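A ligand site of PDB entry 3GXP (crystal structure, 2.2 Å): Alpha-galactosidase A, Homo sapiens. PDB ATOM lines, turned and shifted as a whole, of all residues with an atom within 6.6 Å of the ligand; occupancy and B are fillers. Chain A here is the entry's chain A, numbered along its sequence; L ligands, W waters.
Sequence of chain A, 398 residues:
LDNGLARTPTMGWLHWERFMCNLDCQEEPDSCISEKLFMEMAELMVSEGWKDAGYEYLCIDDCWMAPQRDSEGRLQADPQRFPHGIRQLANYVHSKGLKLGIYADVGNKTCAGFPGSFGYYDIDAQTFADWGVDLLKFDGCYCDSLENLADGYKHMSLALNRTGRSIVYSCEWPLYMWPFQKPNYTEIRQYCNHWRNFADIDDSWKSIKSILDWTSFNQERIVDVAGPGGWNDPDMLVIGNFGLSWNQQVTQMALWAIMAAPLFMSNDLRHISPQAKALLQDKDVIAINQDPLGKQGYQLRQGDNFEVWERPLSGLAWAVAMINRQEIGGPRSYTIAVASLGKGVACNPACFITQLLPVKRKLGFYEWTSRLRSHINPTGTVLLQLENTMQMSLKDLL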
ATOM      1  N   LEU A  14      -2.520  -5.108   0.947  1.00  0.00           N
ATOM      2  CA  LEU A  14      -1.462  -4.094   0.990  1.00  0.00           C
ATOM      3  C   LEU A  14      -1.866  -2.886   0.153  1.00  0.00           C
ATOM      4  O   LEU A  14      -2.146  -3.066  -1.045  1.00  0.00           O
ATOM      5  CB  LEU A  14      -0.190  -4.664   0.373  1.00  0.00           C
ATOM      6  CG  LEU A  14       1.211  -4.295   0.877  1.00  0.00           C
ATOM      7  CD1 LEU A  14       2.059  -4.200  -0.352  1.00  0.00           C
ATOM      8  CD2 LEU A  14       1.328  -3.016   1.686  1.00  0.00           C
ATOM      9  N   TRP A  16      -0.533  -0.105  -1.310  1.00  0.00           N
ATOM     10  CA  TRP A  16       0.147   0.739  -2.309  1.00  0.00           C
ATOM     11  C   TRP A  16      -0.444   0.857  -3.727  1.00  0.00           C
ATOM     12  O   TRP A  16      -0.596   1.965  -4.226  1.00  0.00           O
ATOM     13  CB  TRP A  16       1.601   0.331  -2.464  1.00  0.00           C
ATOM     14  CG  TRP A  16       2.314   1.320  -3.354  1.00  0.00           C
ATOM     15  CD1 TRP A  16       2.694   1.115  -4.641  1.00  0.00           C
ATOM     16  CD2 TRP A  16       2.705   2.667  -3.032  1.00  0.00           C
ATOM     17  NE1 TRP A  16       3.318   2.238  -5.130  1.00  0.00           N
ATOM     18  CE2 TRP A  16       3.325   3.200  -4.166  1.00  0.00           C
ATOM     19  CE3 TRP A  16       2.551   3.481  -1.891  1.00  0.00           C
ATOM     20  CZ2 TRP A  16       3.826   4.511  -4.205  1.00  0.00           C
ATOM     21  CZ3 TRP A  16       3.058   4.784  -1.926  1.00  0.00           C
ATOM     22  CH2 TRP A  16       3.685   5.290  -3.070  1.00  0.00           C
ATOM     23  N   CYS A  21       0.247   7.069  -2.604  1.00  0.00           N
ATOM     24  CA  CYS A  21       0.624   8.033  -1.575  1.00  0.00           C
ATOM     25  C   CYS A  21      -0.365   9.205  -1.484  1.00  0.00           C
ATOM     26  O   CYS A  21       0.040  10.359  -1.604  1.00  0.00           O
ATOM     27  CB  CYS A  21       2.021   8.578  -1.871  1.00  0.00           C
ATOM     28  SG  CYS A  21       2.733   9.424  -0.485  1.00  0.00           S
ATOM     29  N   ASP A  61       1.692   0.281   3.430  1.00  0.00           N
ATOM     30  CA  ASP A  61       2.860   0.477   2.588  1.00  0.00           C
ATOM     31  C   ASP A  61       3.391   1.867   2.946  1.00  0.00           C
ATOM     32  O   ASP A  61       3.225   2.328   4.118  1.00  0.00           O
ATOM     33  CB  ASP A  61       2.471   0.326   1.112  1.00  0.00           C
ATOM     34  CG  ASP A  61       3.656  -0.099   0.207  1.00  0.00           C
ATOM     35  OD1 ASP A  61       4.510   0.787  -0.110  1.00  0.00           O
ATOM     36  OD2 ASP A  61       3.658  -1.288  -0.252  1.00  0.00           O
ATOM     37  N   ASP A  62       4.012   2.548   1.981  1.00  0.00           N
ATOM     38  CA  ASP A  62       4.653   3.837   2.211  1.00  0.00           C
ATOM     39  C   ASP A  62       3.570   4.871   2.551  1.00  0.00           C
ATOM     40  O   ASP A  62       2.346   4.579   2.466  1.00  0.00           O
ATOM     41  CB  ASP A  62       5.456   4.246   0.970  1.00  0.00           C
ATOM     42  CG  ASP A  62       6.647   5.177   1.261  1.00  0.00           C
ATOM     43  OD1 ASP A  62       6.782   5.857   2.345  1.00  0.00           O
ATOM     44  OD2 ASP A  62       7.471   5.252   0.330  1.00  0.00           O
ATOM     45  N   CYS A  63       4.040   6.047   2.986  1.00  0.00           N
ATOM     46  CA  CYS A  63       3.246   7.219   3.323  1.00  0.00           C
ATOM     47  C   CYS A  63       2.414   7.165   4.604  1.00  0.00           C
ATOM     48  O   CYS A  63       1.361   7.753   4.702  1.00  0.00           O
ATOM     49  CB  CYS A  63       2.459   7.773   2.105  1.00  0.00           C
ATOM     50  SG  CYS A  63       3.543   7.981   0.669  1.00  0.00           S
ATOM     51  N   TYR A 103       5.637  -0.593   6.829  1.00  0.00           N
ATOM     52  CA  TYR A 103       6.597  -0.451   5.717  1.00  0.00           C
ATOM     53  C   TYR A 103       7.714   0.489   6.146  1.00  0.00           C
ATOM     54  O   TYR A 103       7.435   1.558   6.677  1.00  0.00           O
ATOM     55  CB  TYR A 103       5.874   0.182   4.487  1.00  0.00           C
ATOM     56  CG  TYR A 103       6.793   0.829   3.450  1.00  0.00           C
ATOM     57  CD1 TYR A 103       7.086   0.181   2.230  1.00  0.00           C
ATOM     58  CD2 TYR A 103       7.386   2.085   3.697  1.00  0.00           C
ATOM     59  CE1 TYR A 103       7.953   0.797   1.273  1.00  0.00           C
ATOM     60  CE2 TYR A 103       8.272   2.697   2.755  1.00  0.00           C
ATOM     61  CZ  TYR A 103       8.546   2.044   1.557  1.00  0.00           C
ATOM     62  OH  TYR A 103       9.413   2.646   0.682  1.00  0.00           O
ATOM     63  N   THR A 110      12.424   6.722   2.633  1.00  0.00           N
ATOM     64  CA  THR A 110      11.494   5.837   1.970  1.00  0.00           C
ATOM     65  C   THR A 110      11.260   6.360   0.530  1.00  0.00           C
ATOM     66  O   THR A 110      11.480   7.530   0.234  1.00  0.00           O
ATOM     67  CB  THR A 110      10.116   5.743   2.729  1.00  0.00           C
ATOM     68  OG1 THR A 110       9.429   6.980   2.632  1.00  0.00           O
ATOM     69  CG2 THR A 110      10.240   5.345   4.179  1.00  0.00           C
ATOM     70  N   CYS A 111      10.794   5.505  -0.360  1.00  0.00           N
ATOM     71  CA  CYS A 111      10.697   5.880  -1.764  1.00  0.00           C
ATOM     72  C   CYS A 111       9.902   7.173  -2.008  1.00  0.00           C
ATOM     73  O   CYS A 111      10.235   7.951  -2.934  1.00  0.00           O
ATOM     74  CB  CYS A 111      10.129   4.713  -2.586  1.00  0.00           C
ATOM     75  SG  CYS A 111      11.282   3.380  -2.687  1.00  0.00           S
ATOM     76  N   ALA A 112       8.840   7.383  -1.226  1.00  0.00           N
ATOM     77  CA  ALA A 112       8.083   8.644  -1.245  1.00  0.00           C
ATOM     78  C   ALA A 112       8.845   9.823  -0.583  1.00  0.00           C
ATOM     79  O   ALA A 112       8.409  10.964  -0.713  1.00  0.00           O
ATOM     80  CB  ALA A 112       6.733   8.483  -0.629  1.00  0.00           C
ATOM     81  N   GLY A 113       9.960   9.555   0.112  1.00  0.00           N
ATOM     82  CA  GLY A 113      10.783  10.629   0.716  1.00  0.00           C
ATOM     83  C   GLY A 113      10.612  10.859   2.219  1.00  0.00           C
ATOM     84  O   GLY A 113      10.984  11.909   2.712  1.00  0.00           O
ATOM     85  N   LYS A 137       7.623  -4.700   5.604  1.00  0.00           N
ATOM     86  CA  LYS A 137       8.054  -4.599   4.213  1.00  0.00           C
ATOM     87  C   LYS A 137       9.157  -3.548   4.171  1.00  0.00           C
ATOM     88  O   LYS A 137       8.959  -2.385   4.557  1.00  0.00           O
ATOM     89  CB  LYS A 137       6.888  -4.163   3.323  1.00  0.00           C
ATOM     90  CG  LYS A 137       7.205  -4.256   1.808  1.00  0.00           C
ATOM     91  CD  LYS A 137       6.069  -3.694   0.916  1.00  0.00           C
ATOM     92  CE  LYS A 137       6.661  -3.039  -0.347  1.00  0.00           C
ATOM     93  NZ  LYS A 137       5.667  -2.487  -1.280  1.00  0.00           N
ATOM     94  N   ASP A 139      11.998  -1.472   2.093  1.00  0.00           N
ATOM     95  CA  ASP A 139      12.201  -1.066   0.710  1.00  0.00           C
ATOM     96  C   ASP A 139      13.641  -0.532   0.621  1.00  0.00           C
ATOM     97  O   ASP A 139      14.247  -0.294   1.658  1.00  0.00           O
ATOM     98  CB  ASP A 139      11.137  -0.015   0.403  1.00  0.00           C
ATOM     99  CG  ASP A 139      10.890   0.173  -1.078  1.00  0.00           C
ATOM    100  OD1 ASP A 139      11.640  -0.377  -1.954  1.00  0.00           O
ATOM    101  OD2 ASP A 139       9.903   0.889  -1.358  1.00  0.00           O
ATOM    102  N   CYS A 141      15.146   2.209  -1.606  1.00  0.00           N
ATOM    103  CA  CYS A 141      15.423   3.603  -2.037  1.00  0.00           C
ATOM    104  C   CYS A 141      16.407   4.303  -1.161  1.00  0.00           C
ATOM    105  O   CYS A 141      16.496   4.007   0.025  1.00  0.00           O
ATOM    106  CB  CYS A 141      14.129   4.452  -1.991  1.00  0.00           C
ATOM    107  SG  CYS A 141      13.036   4.194  -3.419  1.00  0.00           S
ATOM    108  N   GLU A 172      13.151  -5.925  -0.345  1.00  0.00           N
ATOM    109  CA  GLU A 172      13.250  -5.549  -1.721  1.00  0.00           C
ATOM    110  C   GLU A 172      14.670  -5.572  -2.177  1.00  0.00           C
ATOM    111  O   GLU A 172      15.010  -5.022  -3.217  1.00  0.00           O
ATOM    112  CB  GLU A 172      12.600  -4.208  -1.952  1.00  0.00           C
ATOM    113  CG  GLU A 172      11.076  -4.219  -1.660  1.00  0.00           C
ATOM    114  CD  GLU A 172      10.350  -3.114  -2.373  1.00  0.00           C
ATOM    115  OE1 GLU A 172      10.504  -3.005  -3.612  1.00  0.00           O
ATOM    116  OE2 GLU A 172       9.591  -2.368  -1.707  1.00  0.00           O
ATOM    117  N   LEU A 175      15.677  -6.705  -6.065  1.00  0.00           N
ATOM    118  CA  LEU A 175      15.259  -5.662  -7.002  1.00  0.00           C
ATOM    119  C   LEU A 175      16.270  -4.497  -7.135  1.00  0.00           C
ATOM    120  O   LEU A 175      16.484  -3.968  -8.251  1.00  0.00           O
ATOM    121  CB  LEU A 175      13.896  -5.110  -6.619  1.00  0.00           C
ATOM    122  CG  LEU A 175      13.382  -3.897  -7.398  1.00  0.00           C
ATOM    123  CD1 LEU A 175      13.197  -4.274  -8.883  1.00  0.00           C
ATOM    124  CD2 LEU A 175      12.115  -3.347  -6.772  1.00  0.00           C
ATOM    125  N   TYR A 176      16.847  -4.088  -5.997  1.00  0.00           N
ATOM    126  CA  TYR A 176      17.737  -2.897  -5.962  1.00  0.00           C
ATOM    127  C   TYR A 176      19.175  -3.293  -6.310  1.00  0.00           C
ATOM    128  O   TYR A 176      20.014  -2.458  -6.565  1.00  0.00           O
ATOM    129  CB  TYR A 176      17.611  -2.123  -4.617  1.00  0.00           C
ATOM    130  CG  TYR A 176      16.335  -1.330  -4.492  1.00  0.00           C
ATOM    131  CD1 TYR A 176      16.286   0.028  -4.826  1.00  0.00           C
ATOM    132  CD2 TYR A 176      15.140  -1.981  -4.113  1.00  0.00           C
ATOM    133  CE1 TYR A 176      15.079   0.738  -4.755  1.00  0.00           C
ATOM    134  CE2 TYR A 176      13.929  -1.284  -4.059  1.00  0.00           C
ATOM    135  CZ  TYR A 176      13.897   0.035  -4.386  1.00  0.00           C
ATOM    136  OH  TYR A 176      12.686   0.646  -4.277  1.00  0.00           O
ATOM    137  N   ARG A 196      11.112  -9.130  -3.187  1.00  0.00           N
ATOM    138  CA  ARG A 196      10.715  -8.567  -4.494  1.00  0.00           C
ATOM    139  C   ARG A 196      11.877  -8.613  -5.511  1.00  0.00           C
ATOM    140  O   ARG A 196      13.014  -8.195  -5.207  1.00  0.00           O
ATOM    141  CB  ARG A 196      10.246  -7.099  -4.357  1.00  0.00           C
ATOM    142  CG  ARG A 196       8.888  -6.847  -3.680  1.00  0.00           C
ATOM    143  CD  ARG A 196       7.728  -6.978  -4.678  1.00  0.00           C
ATOM    144  NE  ARG A 196       8.090  -6.226  -5.862  1.00  0.00           N
ATOM    145  CZ  ARG A 196       7.977  -4.913  -6.013  1.00  0.00           C
ATOM    146  NH1 ARG A 196       7.423  -4.156  -5.072  1.00  0.00           N
ATOM    147  NH2 ARG A 196       8.427  -4.351  -7.108  1.00  0.00           N
ATOM    148  N   PHE A 198      11.530  -7.764  -9.122  1.00  0.00           N
ATOM    149  CA  PHE A 198      11.192  -7.056 -10.390  1.00  0.00           C
ATOM    150  C   PHE A 198      10.380  -5.808 -10.042  1.00  0.00           C
ATOM    151  O   PHE A 198       9.912  -5.669  -8.894  1.00  0.00           O
ATOM    152  CB  PHE A 198      10.344  -8.000 -11.300  1.00  0.00           C
ATOM    153  CG  PHE A 198      10.167  -7.485 -12.739  1.00  0.00           C
ATOM    154  CD1 PHE A 198      11.278  -7.194 -13.552  1.00  0.00           C
ATOM    155  CD2 PHE A 198       8.892  -7.221 -13.261  1.00  0.00           C
ATOM    156  CE1 PHE A 198      11.112  -6.701 -14.807  1.00  0.00           C
ATOM    157  CE2 PHE A 198       8.771  -6.747 -14.491  1.00  0.00           C
ATOM    158  CZ  PHE A 198       9.873  -6.502 -15.265  1.00  0.00           C
ATOM    159  N   ALA A 199      10.224  -4.935 -11.057  1.00  0.00           N
ATOM    160  CA  ALA A 199       9.516  -3.622 -11.002  1.00  0.00           C
ATOM    161  C   ALA A 199       8.092  -3.710 -10.480  1.00  0.00           C
ATOM    162  O   ALA A 199       7.364  -4.688 -10.761  1.00  0.00           O
ATOM    163  CB  ALA A 199       9.506  -2.898 -12.381  1.00  0.00           C
ATOM    164  N   ASP A 200       7.725  -2.680  -9.740  1.00  0.00           N
ATOM    165  CA  ASP A 200       6.381  -2.513  -9.222  1.00  0.00           C
ATOM    166  C   ASP A 200       5.330  -2.870 -10.256  1.00  0.00           C
ATOM    167  O   ASP A 200       5.427  -2.440 -11.393  1.00  0.00           O
ATOM    168  CB  ASP A 200       6.206  -1.085  -8.755  1.00  0.00           C
ATOM    169  CG  ASP A 200       7.113  -0.763  -7.598  1.00  0.00           C
ATOM    170  OD1 ASP A 200       7.847  -1.651  -7.112  1.00  0.00           O
ATOM    171  OD2 ASP A 200       7.112   0.389  -7.157  1.00  0.00           O
ATOM    172  N   ILE A 201       4.363  -3.689  -9.842  1.00  0.00           N
ATOM    173  CA  ILE A 201       3.136  -3.946 -10.615  1.00  0.00           C
ATOM    174  C   ILE A 201       2.276  -2.695 -10.830  1.00  0.00           C
ATOM    175  O   ILE A 201       2.283  -1.769  -9.960  1.00  0.00           O
ATOM    176  CB  ILE A 201       2.342  -5.152  -9.998  1.00  0.00           C
ATOM    177  CG1 ILE A 201       1.637  -5.963 -11.114  1.00  0.00           C
ATOM    178  CG2 ILE A 201       1.440  -4.717  -8.816  1.00  0.00           C
ATOM    179  CD1 ILE A 201       0.888  -7.209 -10.649  1.00  0.00           C
ATOM    180  N   ASP A 235       5.104  -9.373  -6.670  1.00  0.00           N
ATOM    181  CA  ASP A 235       4.308  -8.193  -6.315  1.00  0.00           C
ATOM    182  C   ASP A 235       2.801  -8.530  -6.151  1.00  0.00           C
ATOM    183  O   ASP A 235       2.369  -9.730  -6.179  1.00  0.00           O
ATOM    184  CB  ASP A 235       4.548  -6.959  -7.253  1.00  0.00           C
ATOM    185  CG  ASP A 235       4.542  -5.621  -6.507  1.00  0.00           C
ATOM    186  OD1 ASP A 235       4.168  -5.573  -5.309  1.00  0.00           O
ATOM    187  OD2 ASP A 235       4.913  -4.609  -7.108  1.00  0.00           O
ATOM    188  N   MET A 236       2.055  -7.454  -5.910  1.00  0.00           N
ATOM    189  CA  MET A 236       0.682  -7.466  -5.411  1.00  0.00           C
ATOM    190  C   MET A 236      -0.242  -8.035  -6.460  1.00  0.00           C
ATOM    191  O   MET A 236       0.014  -7.901  -7.662  1.00  0.00           O
ATOM    192  CB  MET A 236       0.253  -6.026  -5.094  1.00  0.00           C
ATOM    193  CG  MET A 236       0.813  -5.523  -3.778  1.00  0.00           C
ATOM    194  SD  MET A 236       0.631  -3.678  -3.675  1.00  0.00           S
ATOM    195  CE  MET A 236       1.908  -3.079  -4.804  1.00  0.00           C
HETATM  196  C1  LIG L   1       8.626   1.159  -4.057  1.00  0.00           C
HETATM  197  C2  LIG L   1       8.126  -0.281  -3.858  1.00  0.00           C
HETATM  198  C3  LIG L   1       6.603  -0.253  -4.061  1.00  0.00           C
HETATM  199  C4  LIG L   1       6.069   0.742  -3.027  1.00  0.00           C
HETATM  200  C5  LIG L   1       6.683   2.133  -3.157  1.00  0.00           C
HETATM  201  C6  LIG L   1       6.459   2.998  -1.884  1.00  0.00           C
HETATM  202  O1  LIG L   1       8.392   1.790  -5.291  1.00  0.00           O
HETATM  203  O2  LIG L   1       8.923  -1.118  -4.732  1.00  0.00           O
HETATM  204  O3  LIG L   1       5.915  -1.487  -3.863  1.00  0.00           O
HETATM  205  O4  LIG L   1       6.271   0.299  -1.710  1.00  0.00           O
HETATM  206  O5  LIG L   1       8.026   2.014  -3.151  1.00  0.00           O
HETATM  207  O6  LIG L   1       6.886   4.373  -2.057  1.00  0.00           O
HETATM  208  O   HOH W   1       4.712  -2.257  -6.047  1.00  0.00           O
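The side-chain carboxylate of Asp 61 is in salt-bridge range of the side-chain amino group of Lys 137 (2.6 Å).
N of Ala 112 sits at hydrogen-bond distance from OD2 of Asp 62 (3.0 Å).
OE2 of Glu 172 lies within salt-bridge range of NZ of Lys 137 (3.9 Å).
The guanidinium group (NH1) of Arg 196 is in salt-bridge range of the side-chain carboxylate (OE1) of Glu 172, at 3.6 Å.
The side-chain carboxylate of Asp 139 is in hydrogen-bond range of the side-chain hydroxyl of Tyr 103 (2.7 Å).
The backbone NH (N) of Leu 175 is in hydrogen-bond range of the backbone carbonyl oxygen (O) of Arg 196.
NH1 of Arg 196 is in salt-bridge range of OD2 of Asp 235, at 3.3 Å.
The side-chain sulfur (SG) of Cys 63 forms a disulfide with the side-chain sulfur (SG) of Cys 21, 2.0 Å away.
Water W1 lies within hydrogen-bond range of OD2 of Asp 235 (2.6 Å), O3 of the ligand (2.6 Å), OD1 of Asp 200 (3.4 Å) and NH1 of Arg 196 (3.5 Å).
SG of Cys 111 lies close to O5 of the ligand, at 3.6 Å.
OD2 of Asp 139 lies close to O5 of the ligand, at 2.8 Å.
Merely in contact with the ligand: Tyr 103, Trp 16 and Ala 112.
Within 4 Å of the ligand: Trp 16, Asp 61, Asp 62, Tyr 103, Cys 111, Ala 112, Lys 137, Asp 139, Glu 172, Arg 196 and Asp 200.
Along chain A the residues within 4 Å of the ligand span positions 16 to 200.
OD1 of Asp 61 is in hydrogen-bond range of O4 of the ligand, 2.4 Å away.
OD2 of Asp 62 lies within hydrogen-bond range of O6 of the ligand, at 2.6 Å.
The side-chain carboxylate (OD2) of Asp 200 lies within hydrogen-bond range of an oxygen (O1) of the ligand, at 2.7 Å.
OE1 of Glu 172 lies within hydrogen-bond range of O2 of the ligand.
An oxygen (O3) of the ligand lies within hydrogen-bond range of the side-chain amino group (NZ) of Lys 137 (2.8 Å).
NH1 of Arg 196 is in hydrogen-bond range of O3 of the ligand, 3.3 Å away.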
